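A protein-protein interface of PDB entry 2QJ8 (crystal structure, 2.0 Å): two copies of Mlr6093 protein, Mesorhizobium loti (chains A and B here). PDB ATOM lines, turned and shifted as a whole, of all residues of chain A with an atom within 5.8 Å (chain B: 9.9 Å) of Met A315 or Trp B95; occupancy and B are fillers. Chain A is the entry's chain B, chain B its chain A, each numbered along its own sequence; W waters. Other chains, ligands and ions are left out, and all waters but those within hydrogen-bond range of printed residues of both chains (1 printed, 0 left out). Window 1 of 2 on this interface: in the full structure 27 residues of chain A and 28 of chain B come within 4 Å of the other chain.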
ATOM      1  N   THR A 146     -10.137  -7.455  -6.065  1.00  0.00           N
ATOM      2  CA  THR A 146      -9.352  -6.669  -7.016  1.00  0.00           C
ATOM      3  C   THR A 146      -7.960  -7.221  -7.341  1.00  0.00           C
ATOM      4  O   THR A 146      -7.215  -6.562  -8.062  1.00  0.00           O
ATOM      5  CB  THR A 146      -9.175  -5.233  -6.489  1.00  0.00           C
ATOM      6  OG1 THR A 146      -8.291  -5.223  -5.360  1.00  0.00           O
ATOM      7  CG2 THR A 146     -10.519  -4.610  -6.123  1.00  0.00           C
ATOM      8  N   GLY A 266      -3.621   6.844 -11.251  1.00  0.00           N
ATOM      9  CA  GLY A 266      -4.196   6.527 -12.536  1.00  0.00           C
ATOM     10  C   GLY A 266      -4.839   5.162 -12.603  1.00  0.00           C
ATOM     11  O   GLY A 266      -4.955   4.432 -11.586  1.00  0.00           O
ATOM     12  N   ILE A 267      -5.259   4.838 -13.816  1.00  0.00           N
ATOM     13  CA  ILE A 267      -5.911   3.572 -14.120  1.00  0.00           C
ATOM     14  C   ILE A 267      -4.863   2.545 -14.456  1.00  0.00           C
ATOM     15  O   ILE A 267      -4.210   2.640 -15.489  1.00  0.00           O
ATOM     16  CB  ILE A 267      -6.931   3.724 -15.292  1.00  0.00           C
ATOM     17  CG1 ILE A 267      -8.069   4.678 -14.874  1.00  0.00           C
ATOM     18  CG2 ILE A 267      -7.494   2.366 -15.676  1.00  0.00           C
ATOM     19  CD1 ILE A 267      -9.037   5.037 -16.001  1.00  0.00           C
ATOM     20  N   PHE A 268      -4.710   1.546 -13.584  1.00  0.00           N
ATOM     21  CA  PHE A 268      -3.742   0.471 -13.799  1.00  0.00           C
ATOM     22  C   PHE A 268      -4.384  -0.589 -14.682  1.00  0.00           C
ATOM     23  O   PHE A 268      -5.527  -0.934 -14.450  1.00  0.00           O
ATOM     24  CB  PHE A 268      -3.355  -0.173 -12.471  1.00  0.00           C
ATOM     25  CG  PHE A 268      -2.506  -1.391 -12.623  1.00  0.00           C
ATOM     26  CD1 PHE A 268      -1.174  -1.268 -13.000  1.00  0.00           C
ATOM     27  CD2 PHE A 268      -3.033  -2.665 -12.388  1.00  0.00           C
ATOM     28  CE1 PHE A 268      -0.378  -2.394 -13.157  1.00  0.00           C
ATOM     29  CE2 PHE A 268      -2.234  -3.792 -12.539  1.00  0.00           C
ATOM     30  CZ  PHE A 268      -0.913  -3.654 -12.921  1.00  0.00           C
ATOM     31  N   GLU A 269      -3.663  -1.051 -15.694  1.00  0.00           N
ATOM     32  CA  GLU A 269      -4.111  -2.102 -16.574  1.00  0.00           C
ATOM     33  C   GLU A 269      -3.068  -3.221 -16.489  1.00  0.00           C
ATOM     34  O   GLU A 269      -1.933  -3.003 -16.894  1.00  0.00           O
ATOM     35  CB  GLU A 269      -4.199  -1.595 -18.014  1.00  0.00           C
ATOM     36  CG  GLU A 269      -4.521  -2.708 -18.995  1.00  0.00           C
ATOM     37  CD  GLU A 269      -4.405  -2.315 -20.419  1.00  0.00           C
ATOM     38  OE1 GLU A 269      -4.171  -1.129 -20.751  1.00  0.00           O
ATOM     39  OE2 GLU A 269      -4.555  -3.259 -21.219  1.00  0.00           O
ATOM     40  N   ARG A 312      -2.932  -7.084  -9.760  1.00  0.00           N
ATOM     41  CA  ARG A 312      -4.131  -6.322  -9.529  1.00  0.00           C
ATOM     42  C   ARG A 312      -4.951  -6.338 -10.821  1.00  0.00           C
ATOM     43  O   ARG A 312      -4.402  -6.457 -11.938  1.00  0.00           O
ATOM     44  CB  ARG A 312      -3.733  -4.909  -9.119  1.00  0.00           C
ATOM     45  CG  ARG A 312      -4.780  -4.179  -8.400  1.00  0.00           C
ATOM     46  CD  ARG A 312      -4.403  -2.720  -8.125  1.00  0.00           C
ATOM     47  NE  ARG A 312      -3.722  -2.433  -6.854  1.00  0.00           N
ATOM     48  CZ  ARG A 312      -4.288  -2.488  -5.644  1.00  0.00           C
ATOM     49  NH1 ARG A 312      -5.544  -2.900  -5.469  1.00  0.00           N
ATOM     50  NH2 ARG A 312      -3.573  -2.174  -4.566  1.00  0.00           N
ATOM     51  N   SER A 313      -6.265  -6.291 -10.667  1.00  0.00           N
ATOM     52  CA  SER A 313      -7.161  -6.140 -11.810  1.00  0.00           C
ATOM     53  C   SER A 313      -7.096  -4.669 -12.259  1.00  0.00           C
ATOM     54  O   SER A 313      -6.438  -3.845 -11.630  1.00  0.00           O
ATOM     55  CB  SER A 313      -8.585  -6.500 -11.432  1.00  0.00           C
ATOM     56  OG  SER A 313      -8.648  -7.828 -10.940  1.00  0.00           O
ATOM     57  N   ALA A 314      -7.758  -4.361 -13.368  1.00  0.00           N
ATOM     58  CA  ALA A 314      -7.797  -3.014 -13.892  1.00  0.00           C
ATOM     59  C   ALA A 314      -8.603  -2.138 -12.927  1.00  0.00           C
ATOM     60  O   ALA A 314      -9.733  -2.484 -12.576  1.00  0.00           O
ATOM     61  CB  ALA A 314      -8.392  -3.004 -15.306  1.00  0.00           C
ATOM     62  N   MET A 315      -8.007  -1.046 -12.442  1.00  0.00           N
ATOM     63  CA  MET A 315      -8.639  -0.157 -11.470  1.00  0.00           C
ATOM     64  C   MET A 315      -7.863   1.121 -11.237  1.00  0.00           C
ATOM     65  O   MET A 315      -6.700   1.202 -11.564  1.00  0.00           O
ATOM     66  CB  MET A 315      -8.800  -0.830 -10.126  1.00  0.00           C
ATOM     67  CG  MET A 315      -7.534  -1.192  -9.451  1.00  0.00           C
ATOM     68  SD  MET A 315      -8.007  -2.181  -7.867  1.00  0.00           S
ATOM     69  CE  MET A 315      -9.060  -0.864  -6.873  1.00  0.00           C
ATOM     70  N   TYR A 316      -8.509   2.089 -10.596  1.00  0.00           N
ATOM     71  CA  TYR A 316      -7.857   3.340 -10.281  1.00  0.00           C
ATOM     72  C   TYR A 316      -6.983   3.079  -9.072  1.00  0.00           C
ATOM     73  O   TYR A 316      -7.456   2.529  -8.096  1.00  0.00           O
ATOM     74  CB  TYR A 316      -8.853   4.438  -9.948  1.00  0.00           C
ATOM     75  CG  TYR A 316      -8.193   5.756  -9.659  1.00  0.00           C
ATOM     76  CD1 TYR A 316      -7.545   6.445 -10.658  1.00  0.00           C
ATOM     77  CD2 TYR A 316      -8.197   6.306  -8.384  1.00  0.00           C
ATOM     78  CE1 TYR A 316      -6.929   7.658 -10.427  1.00  0.00           C
ATOM     79  CE2 TYR A 316      -7.575   7.497  -8.143  1.00  0.00           C
ATOM     80  CZ  TYR A 316      -6.931   8.165  -9.166  1.00  0.00           C
ATOM     81  OH  TYR A 316      -6.342   9.378  -8.943  1.00  0.00           O
ATOM     82  N   VAL A 317      -5.712   3.444  -9.166  1.00  0.00           N
ATOM     83  CA  VAL A 317      -4.732   3.284  -8.067  1.00  0.00           C
ATOM     84  C   VAL A 317      -4.104   4.650  -7.813  1.00  0.00           C
ATOM     85  O   VAL A 317      -4.074   5.510  -8.695  1.00  0.00           O
ATOM     86  CB  VAL A 317      -3.606   2.225  -8.386  1.00  0.00           C
ATOM     87  CG1 VAL A 317      -4.192   0.804  -8.532  1.00  0.00           C
ATOM     88  CG2 VAL A 317      -2.789   2.618  -9.619  1.00  0.00           C
ATOM     89  N   GLN A 318      -3.627   4.839  -6.588  1.00  0.00           N
ATOM     90  CA  GLN A 318      -2.906   6.020  -6.170  1.00  0.00           C
ATOM     91  C   GLN A 318      -1.426   5.710  -6.352  1.00  0.00           C
ATOM     92  O   GLN A 318      -1.074   4.568  -6.627  1.00  0.00           O
ATOM     93  CB  GLN A 318      -3.198   6.282  -4.700  1.00  0.00           C
ATOM     94  CG  GLN A 318      -4.655   6.531  -4.369  1.00  0.00           C
ATOM     95  CD  GLN A 318      -5.169   7.830  -4.929  1.00  0.00           C
ATOM     96  OE1 GLN A 318      -4.400   8.708  -5.286  1.00  0.00           O
ATOM     97  NE2 GLN A 318      -6.477   7.970  -4.974  1.00  0.00           N
ATOM     98  N   GLU A 321       1.033   2.454  -4.646  1.00  0.00           N
ATOM     99  CA  GLU A 321       0.154   1.326  -4.378  1.00  0.00           C
ATOM    100  C   GLU A 321       0.731   0.153  -5.117  1.00  0.00           C
ATOM    101  O   GLU A 321       1.113   0.295  -6.269  1.00  0.00           O
ATOM    102  CB  GLU A 321      -1.272   1.527  -4.886  1.00  0.00           C
ATOM    103  CG  GLU A 321      -2.214   2.275  -3.943  1.00  0.00           C
ATOM    104  CD  GLU A 321      -3.701   1.973  -4.251  1.00  0.00           C
ATOM    105  OE1 GLU A 321      -4.081   0.778  -4.268  1.00  0.00           O
ATOM    106  OE2 GLU A 321      -4.491   2.928  -4.437  1.00  0.00           O
ATOM    107  N   HIS B  55     -20.144   3.922 -14.254  1.00  0.00           N
ATOM    108  CA  HIS B  55     -19.982   3.360 -12.914  1.00  0.00           C
ATOM    109  C   HIS B  55     -18.515   3.242 -12.598  1.00  0.00           C
ATOM    110  O   HIS B  55     -17.725   2.985 -13.471  1.00  0.00           O
ATOM    111  CB  HIS B  55     -20.669   2.016 -12.793  1.00  0.00           C
ATOM    112  CG  HIS B  55     -22.149   2.085 -12.992  1.00  0.00           C
ATOM    113  ND1 HIS B  55     -22.998   2.716 -12.099  1.00  0.00           N
ATOM    114  CD2 HIS B  55     -22.938   1.572 -13.963  1.00  0.00           C
ATOM    115  CE1 HIS B  55     -24.241   2.612 -12.543  1.00  0.00           C
ATOM    116  NE2 HIS B  55     -24.233   1.908 -13.659  1.00  0.00           N
ATOM    117  N   GLY B  56     -18.148   3.385 -11.342  1.00  0.00           N
ATOM    118  CA  GLY B  56     -16.730   3.401 -10.983  1.00  0.00           C
ATOM    119  C   GLY B  56     -15.926   2.137 -10.716  1.00  0.00           C
ATOM    120  O   GLY B  56     -14.686   2.184 -10.598  1.00  0.00           O
ATOM    121  N   ASN B  57     -16.604   1.014 -10.657  1.00  0.00           N
ATOM    122  CA  ASN B  57     -15.942  -0.249 -10.385  1.00  0.00           C
ATOM    123  C   ASN B  57     -15.774  -1.134 -11.658  1.00  0.00           C
ATOM    124  O   ASN B  57     -15.664  -2.349 -11.547  1.00  0.00           O
ATOM    125  CB  ASN B  57     -16.657  -0.942  -9.189  1.00  0.00           C
ATOM    126  CG  ASN B  57     -18.230  -0.941  -9.294  1.00  0.00           C
ATOM    127  OD1 ASN B  57     -18.825  -0.675 -10.357  1.00  0.00           O
ATOM    128  ND2 ASN B  57     -18.885  -1.283  -8.170  1.00  0.00           N
ATOM    129  N   GLU B  58     -15.712  -0.492 -12.827  1.00  0.00           N
ATOM    130  CA  GLU B  58     -15.600  -1.165 -14.113  1.00  0.00           C
ATOM    131  C   GLU B  58     -14.610  -0.400 -14.939  1.00  0.00           C
ATOM    132  O   GLU B  58     -14.926   0.698 -15.416  1.00  0.00           O
ATOM    133  CB  GLU B  58     -16.967  -1.172 -14.808  1.00  0.00           C
ATOM    134  CG  GLU B  58     -17.118  -2.193 -15.946  1.00  0.00           C
ATOM    135  CD  GLU B  58     -16.120  -2.048 -17.066  1.00  0.00           C
ATOM    136  OE1 GLU B  58     -16.058  -0.970 -17.713  1.00  0.00           O
ATOM    137  OE2 GLU B  58     -15.386  -3.031 -17.301  1.00  0.00           O
ATOM    138  N   LEU B  59     -13.413  -0.946 -15.111  1.00  0.00           N
ATOM    139  CA  LEU B  59     -12.403  -0.258 -15.873  1.00  0.00           C
ATOM    140  C   LEU B  59     -12.156  -0.794 -17.258  1.00  0.00           C
ATOM    141  O   LEU B  59     -11.436  -0.146 -17.984  1.00  0.00           O
ATOM    142  CB  LEU B  59     -11.120  -0.132 -15.069  1.00  0.00           C
ATOM    143  CG  LEU B  59     -11.131   0.918 -13.952  1.00  0.00           C
ATOM    144  CD1 LEU B  59     -11.291   2.359 -14.425  1.00  0.00           C
ATOM    145  CD2 LEU B  59     -12.154   0.593 -12.881  1.00  0.00           C
ATOM    146  N   GLN B  60     -12.761  -1.908 -17.651  1.00  0.00           N
ATOM    147  CA  GLN B  60     -12.473  -2.485 -18.984  1.00  0.00           C
ATOM    148  C   GLN B  60     -13.019  -1.592 -20.115  1.00  0.00           C
ATOM    149  O   GLN B  60     -12.372  -1.476 -21.138  1.00  0.00           O
ATOM    150  CB  GLN B  60     -12.928  -3.951 -19.119  1.00  0.00           C
ATOM    151  CG  GLN B  60     -12.419  -4.932 -18.010  1.00  0.00           C
ATOM    152  CD  GLN B  60     -10.886  -5.137 -17.934  1.00  0.00           C
ATOM    153  OE1 GLN B  60     -10.170  -5.066 -18.927  1.00  0.00           O
ATOM    154  NE2 GLN B  60     -10.399  -5.420 -16.727  1.00  0.00           N
ATOM    155  N   GLY B  61     -14.177  -0.960 -19.888  1.00  0.00           N
ATOM    156  CA  GLY B  61     -14.771   0.022 -20.792  1.00  0.00           C
ATOM    157  C   GLY B  61     -13.836   1.208 -21.005  1.00  0.00           C
ATOM    158  O   GLY B  61     -13.494   1.512 -22.134  1.00  0.00           O
ATOM    159  N   PRO B  62     -13.465   1.930 -19.925  1.00  0.00           N
ATOM    160  CA  PRO B  62     -12.453   2.981 -20.031  1.00  0.00           C
ATOM    161  C   PRO B  62     -11.159   2.589 -20.752  1.00  0.00           C
ATOM    162  O   PRO B  62     -10.666   3.370 -21.573  1.00  0.00           O
ATOM    163  CB  PRO B  62     -12.206   3.338 -18.585  1.00  0.00           C
ATOM    164  CG  PRO B  62     -13.571   3.226 -17.985  1.00  0.00           C
ATOM    165  CD  PRO B  62     -14.093   1.949 -18.589  1.00  0.00           C
ATOM    166  N   ILE B  63     -10.660   1.395 -20.485  1.00  0.00           N
ATOM    167  CA  ILE B  63      -9.435   0.883 -21.141  1.00  0.00           C
ATOM    168  C   ILE B  63      -9.664   0.684 -22.638  1.00  0.00           C
ATOM    169  O   ILE B  63      -8.869   1.158 -23.447  1.00  0.00           O
ATOM    170  CB  ILE B  63      -8.945  -0.406 -20.483  1.00  0.00           C
ATOM    171  CG1 ILE B  63      -8.310  -0.077 -19.127  1.00  0.00           C
ATOM    172  CG2 ILE B  63      -7.938  -1.140 -21.391  1.00  0.00           C
ATOM    173  CD1 ILE B  63      -8.265  -1.294 -18.167  1.00  0.00           C
ATOM    174  N   ARG B  66      -9.835   3.995 -24.381  1.00  0.00           N
ATOM    175  CA  ARG B  66      -8.522   4.541 -24.606  1.00  0.00           C
ATOM    176  C   ARG B  66      -7.794   3.829 -25.743  1.00  0.00           C
ATOM    177  O   ARG B  66      -6.987   4.442 -26.443  1.00  0.00           O
ATOM    178  CB  ARG B  66      -7.693   4.450 -23.341  1.00  0.00           C
ATOM    179  CG  ARG B  66      -8.081   5.448 -22.316  1.00  0.00           C
ATOM    180  CD  ARG B  66      -7.556   5.023 -20.991  1.00  0.00           C
ATOM    181  NE  ARG B  66      -8.010   5.933 -19.961  1.00  0.00           N
ATOM    182  CZ  ARG B  66      -7.455   7.099 -19.677  1.00  0.00           C
ATOM    183  NH1 ARG B  66      -6.393   7.558 -20.351  1.00  0.00           N
ATOM    184  NH2 ARG B  66      -8.002   7.831 -18.699  1.00  0.00           N
ATOM    185  N   GLU B  86     -14.230   8.032 -19.378  1.00  0.00           N
ATOM    186  CA  GLU B  86     -14.766   7.986 -18.015  1.00  0.00           C
ATOM    187  C   GLU B  86     -15.703   9.164 -17.816  1.00  0.00           C
ATOM    188  O   GLU B  86     -15.253  10.261 -17.478  1.00  0.00           O
ATOM    189  CB  GLU B  86     -13.666   8.077 -16.935  1.00  0.00           C
ATOM    190  CG  GLU B  86     -12.612   6.998 -16.948  1.00  0.00           C
ATOM    191  CD  GLU B  86     -11.378   7.335 -17.747  1.00  0.00           C
ATOM    192  OE1 GLU B  86     -10.792   8.435 -17.551  1.00  0.00           O
ATOM    193  OE2 GLU B  86     -10.934   6.470 -18.533  1.00  0.00           O
ATOM    194  N   ASN B  88     -17.846   9.339 -15.395  1.00  0.00           N
ATOM    195  CA  ASN B  88     -18.040   9.542 -13.949  1.00  0.00           C
ATOM    196  C   ASN B  88     -16.703   9.372 -13.200  1.00  0.00           C
ATOM    197  O   ASN B  88     -16.518   8.382 -12.467  1.00  0.00           O
ATOM    198  CB  ASN B  88     -19.125   8.583 -13.415  1.00  0.00           C
ATOM    199  CG  ASN B  88     -19.656   8.977 -12.040  1.00  0.00           C
ATOM    200  OD1 ASN B  88     -19.047   9.755 -11.321  1.00  0.00           O
ATOM    201  ND2 ASN B  88     -20.774   8.387 -11.658  1.00  0.00           N
ATOM    202  N   PRO B  89     -15.765  10.326 -13.379  1.00  0.00           N
ATOM    203  CA  PRO B  89     -14.453  10.236 -12.696  1.00  0.00           C
ATOM    204  C   PRO B  89     -14.512  10.166 -11.208  1.00  0.00           C
ATOM    205  O   PRO B  89     -13.673   9.532 -10.614  1.00  0.00           O
ATOM    206  CB  PRO B  89     -13.716  11.508 -13.158  1.00  0.00           C
ATOM    207  CG  PRO B  89     -14.747  12.418 -13.654  1.00  0.00           C
ATOM    208  CD  PRO B  89     -15.842  11.545 -14.213  1.00  0.00           C
ATOM    209  N   LEU B  90     -15.485  10.835 -10.590  1.00  0.00           N
ATOM    210  CA  LEU B  90     -15.653  10.751  -9.161  1.00  0.00           C
ATOM    211  C   LEU B  90     -15.867   9.308  -8.692  1.00  0.00           C
ATOM    212  O   LEU B  90     -15.199   8.872  -7.766  1.00  0.00           O
ATOM    213  CB  LEU B  90     -16.821  11.617  -8.726  1.00  0.00           C
ATOM    214  CG  LEU B  90     -16.651  13.118  -8.775  1.00  0.00           C
ATOM    215  CD1 LEU B  90     -17.990  13.751  -8.456  1.00  0.00           C
ATOM    216  CD2 LEU B  90     -15.596  13.561  -7.766  1.00  0.00           C
ATOM    217  N   ALA B  91     -16.753   8.578  -9.377  1.00  0.00           N
ATOM    218  CA  ALA B  91     -17.046   7.178  -9.084  1.00  0.00           C
ATOM    219  C   ALA B  91     -15.842   6.278  -9.367  1.00  0.00           C
ATOM    220  O   ALA B  91     -15.537   5.392  -8.582  1.00  0.00           O
ATOM    221  CB  ALA B  91     -18.253   6.700  -9.920  1.00  0.00           C
ATOM    222  N   VAL B  92     -15.185   6.496 -10.497  1.00  0.00           N
ATOM    223  CA  VAL B  92     -13.979   5.710 -10.859  1.00  0.00           C
ATOM    224  C   VAL B  92     -12.887   5.835  -9.773  1.00  0.00           C
ATOM    225  O   VAL B  92     -12.304   4.825  -9.303  1.00  0.00           O
ATOM    226  CB  VAL B  92     -13.437   6.120 -12.244  1.00  0.00           C
ATOM    227  CG1 VAL B  92     -12.063   5.418 -12.537  1.00  0.00           C
ATOM    228  CG2 VAL B  92     -14.416   5.773 -13.327  1.00  0.00           C
ATOM    229  N   GLN B  93     -12.681   7.061  -9.299  1.00  0.00           N
ATOM    230  CA  GLN B  93     -11.671   7.323  -8.286  1.00  0.00           C
ATOM    231  C   GLN B  93     -12.066   6.882  -6.881  1.00  0.00           C
ATOM    232  O   GLN B  93     -11.193   6.572  -6.104  1.00  0.00           O
ATOM    233  CB  GLN B  93     -11.253   8.778  -8.305  1.00  0.00           C
ATOM    234  CG  GLN B  93     -10.556   9.167  -9.570  1.00  0.00           C
ATOM    235  CD  GLN B  93     -10.047  10.609  -9.568  1.00  0.00           C
ATOM    236  OE1 GLN B  93     -10.305  11.376  -8.665  1.00  0.00           O
ATOM    237  NE2 GLN B  93      -9.346  10.965 -10.606  1.00  0.00           N
ATOM    238  N   ALA B  94     -13.362   6.853  -6.562  1.00  0.00           N
ATOM    239  CA  ALA B  94     -13.851   6.397  -5.260  1.00  0.00           C
ATOM    240  C   ALA B  94     -14.120   4.885  -5.177  1.00  0.00           C
ATOM    241  O   ALA B  94     -14.432   4.418  -4.074  1.00  0.00           O
ATOM    242  CB  ALA B  94     -15.101   7.161  -4.869  1.00  0.00           C
ATOM    243  N   TRP B  95     -13.947   4.138  -6.290  1.00  0.00           N
ATOM    244  CA  TRP B  95     -14.199   2.695  -6.311  1.00  0.00           C
ATOM    245  C   TRP B  95     -15.657   2.385  -5.928  1.00  0.00           C
ATOM    246  O   TRP B  95     -15.919   1.393  -5.238  1.00  0.00           O
ATOM    247  CB  TRP B  95     -13.189   1.970  -5.381  1.00  0.00           C
ATOM    248  CG  TRP B  95     -11.789   2.434  -5.647  1.00  0.00           C
ATOM    249  CD1 TRP B  95     -11.112   2.244  -6.798  1.00  0.00           C
ATOM    250  CD2 TRP B  95     -10.918   3.195  -4.787  1.00  0.00           C
ATOM    251  NE1 TRP B  95      -9.895   2.822  -6.731  1.00  0.00           N
ATOM    252  CE2 TRP B  95      -9.730   3.414  -5.507  1.00  0.00           C
ATOM    253  CE3 TRP B  95     -11.028   3.714  -3.487  1.00  0.00           C
ATOM    254  CZ2 TRP B  95      -8.638   4.125  -4.977  1.00  0.00           C
ATOM    255  CZ3 TRP B  95      -9.944   4.423  -2.954  1.00  0.00           C
ATOM    256  CH2 TRP B  95      -8.762   4.618  -3.700  1.00  0.00           C
ATOM    257  N   THR B  96     -16.579   3.261  -6.363  1.00  0.00           N
ATOM    258  CA  THR B  96     -17.984   3.192  -6.036  1.00  0.00           C
ATOM    259  C   THR B  96     -18.802   2.922  -7.302  1.00  0.00           C
ATOM    260  O   THR B  96     -18.351   3.214  -8.421  1.00  0.00           O
ATOM    261  CB  THR B  96     -18.398   4.533  -5.382  1.00  0.00           C
ATOM    262  OG1 THR B  96     -17.428   4.913  -4.393  1.00  0.00           O
ATOM    263  CG2 THR B  96     -19.709   4.416  -4.714  1.00  0.00           C
ATOM    264  N   ARG B  97     -19.993   2.361  -7.150  1.00  0.00           N
ATOM    265  CA  ARG B  97     -20.825   2.115  -8.313  1.00  0.00           C
ATOM    266  C   ARG B  97     -21.374   3.421  -8.835  1.00  0.00           C
ATOM    267  O   ARG B  97     -21.317   3.684 -10.008  1.00  0.00           O
ATOM    268  CB  ARG B  97     -21.992   1.186  -8.021  1.00  0.00           C
ATOM    269  CG  ARG B  97     -22.793   0.925  -9.303  1.00  0.00           C
ATOM    270  CD  ARG B  97     -23.442  -0.401  -9.277  1.00  0.00           C
ATOM    271  NE  ARG B  97     -24.017  -0.713 -10.579  1.00  0.00           N
ATOM    272  CZ  ARG B  97     -23.338  -1.139 -11.647  1.00  0.00           C
ATOM    273  NH1 ARG B  97     -22.011  -1.269 -11.651  1.00  0.00           N
ATOM    274  NH2 ARG B  97     -24.008  -1.390 -12.757  1.00  0.00           N
ATOM    275  N   ASN B  98     -21.882   4.249  -7.938  1.00  0.00           N
ATOM    276  CA  ASN B  98     -22.445   5.517  -8.326  1.00  0.00           C
ATOM    277  C   ASN B  98     -21.657   6.699  -7.783  1.00  0.00           C
ATOM    278  O   ASN B  98     -20.686   6.536  -7.036  1.00  0.00           O
ATOM    279  CB  ASN B  98     -23.920   5.492  -7.919  1.00  0.00           C
ATOM    280  CG  ASN B  98     -24.692   4.430  -8.705  1.00  0.00           C
ATOM    281  OD1 ASN B  98     -24.517   4.294  -9.922  1.00  0.00           O
ATOM    282  ND2 ASN B  98     -25.471   3.625  -8.012  1.00  0.00           N
ATOM    283  N   THR B  99     -22.078   7.885  -8.189  1.00  0.00           N
ATOM    284  CA  THR B  99     -21.397   9.103  -7.826  1.00  0.00           C
ATOM    285  C   THR B  99     -21.314   9.230  -6.297  1.00  0.00           C
ATOM    286  O   THR B  99     -22.343   9.236  -5.625  1.00  0.00           O
ATOM    287  CB  THR B  99     -22.122  10.304  -8.430  1.00  0.00           C
ATOM    288  OG1 THR B  99     -22.330  10.068  -9.821  1.00  0.00           O
ATOM    289  CG2 THR B  99     -21.330  11.605  -8.225  1.00  0.00           C
ATOM    290  N   PRO B 100     -20.083   9.293  -5.745  1.00  0.00           N
ATOM    291  CA  PRO B 100     -19.969   9.372  -4.296  1.00  0.00           C
ATOM    292  C   PRO B 100     -20.490  10.661  -3.646  1.00  0.00           C
ATOM    293  O   PRO B 100     -20.902  10.613  -2.485  1.00  0.00           O
ATOM    294  CB  PRO B 100     -18.463   9.225  -4.066  1.00  0.00           C
ATOM    295  CG  PRO B 100     -17.840   9.698  -5.311  1.00  0.00           C
ATOM    296  CD  PRO B 100     -18.756   9.253  -6.388  1.00  0.00           C
ATOM    297  N   PRO B 145     -19.587  -5.459 -11.001  1.00  0.00           N
ATOM    298  CA  PRO B 145     -18.322  -6.226 -10.740  1.00  0.00           C
ATOM    299  C   PRO B 145     -18.502  -7.480  -9.883  1.00  0.00           C
ATOM    300  O   PRO B 145     -17.579  -8.263  -9.728  1.00  0.00           O
ATOM    301  CB  PRO B 145     -17.420  -5.257  -9.972  1.00  0.00           C
ATOM    302  CG  PRO B 145     -18.190  -4.115  -9.691  1.00  0.00           C
ATOM    303  CD  PRO B 145     -19.615  -4.220 -10.208  1.00  0.00           C
HETATM  304  O   HOH W   1     -11.442   2.414 -10.036  1.00  0.00           O
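The backbone carbonyl oxygen (O) of Tyr A316 sits at hydrogen-bond distance from the indole nitrogen (NE1) of Trp B95 (2.8 Å).
The side-chain carboxylate (OE2) of Glu B58 is in hydrogen-bond range of the backbone NH (N) of Gln B60 (2.9 Å). The guanidinium group (NH2) of Arg B66 is in salt-bridge range of the side-chain carboxylate (OE1) of Glu B86 (3.1 Å). The backbone carbonyl oxygen (O) of Met A315 is in hydrogen-bond range of the backbone NH (N) of Phe A268, at 2.9 Å. The side-chain sulfur (SD) of Met A315 lies within hydrogen-bond range of the guanidinium group (NH1) of Arg A312 (3.5 Å).
Among the printed residues, merely in contact across the chains: Ala A314 with Ile B63 (3.3 Å), Ala A314 with Gln B60 (3.4 Å), Ile A267 with Glu B86 (3.5 Å), Tyr A316 with Val B92 (3.5 Å), Tyr A316 with Gln B93 (3.6 Å), Met A315 with Leu B59 (3.7 Å), Ala A314 with Leu B59 (3.7 Å), Met A315 with Trp B95 (3.7 Å), Glu A269 with Ile B63 (3.8 Å) and Ile A267 with Leu B59 (3.8 Å).
Printed residues of chain B within 4 Å of Met A315: Leu B59 (3.7 Å) and Trp B95 (3.7 Å). Printed residues of chain A within 4 Å of Trp B95: Met A315 and Tyr A316. Of chain B, only Leu B59 (3.7 Å), Gln B60 (3.4 Å) and Ile B63 (3.3 Å) come within 4 Å of Ala A314. No residue of chain B comes within 4 Å of Val A317. Printed residues of chain A within 4 Å of Leu B59: Ile A267 (3.8 Å), Ala A314 (3.7 Å) and Met A315 (3.7 Å). Printed residues of chain A within 4 Å of Glu B86: Ile A267. Gln A318 touches none of the printed residues of chain B. The nearest printed residue of chain B that does not touch Met A315 is Ile B63 (5.7 Å).
Printed residues of chain A that touch a printed residue of chain B: Ile A267, Glu A269, Ala A314, Met A315 and Tyr A316. Hydrophobic or aromatic side chains of chain B within 4 Å of the printed part of chain A: Leu B59, Ile B63 and Trp B95. Among the printed residues, no Asp or Glu carboxylate lies within 4 Å of a Lys or Arg side-chain nitrogen of the other chain.
No position is printed for both chains.
Water W1 lies within hydrogen-bond range of the backbone carbonyl oxygen (O) of Val B92 (2.7 Å), the backbone NH (N) of Tyr A316 (3.0 Å) and the backbone carbonyl oxygen (O) of Gly B56 (3.3 Å).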
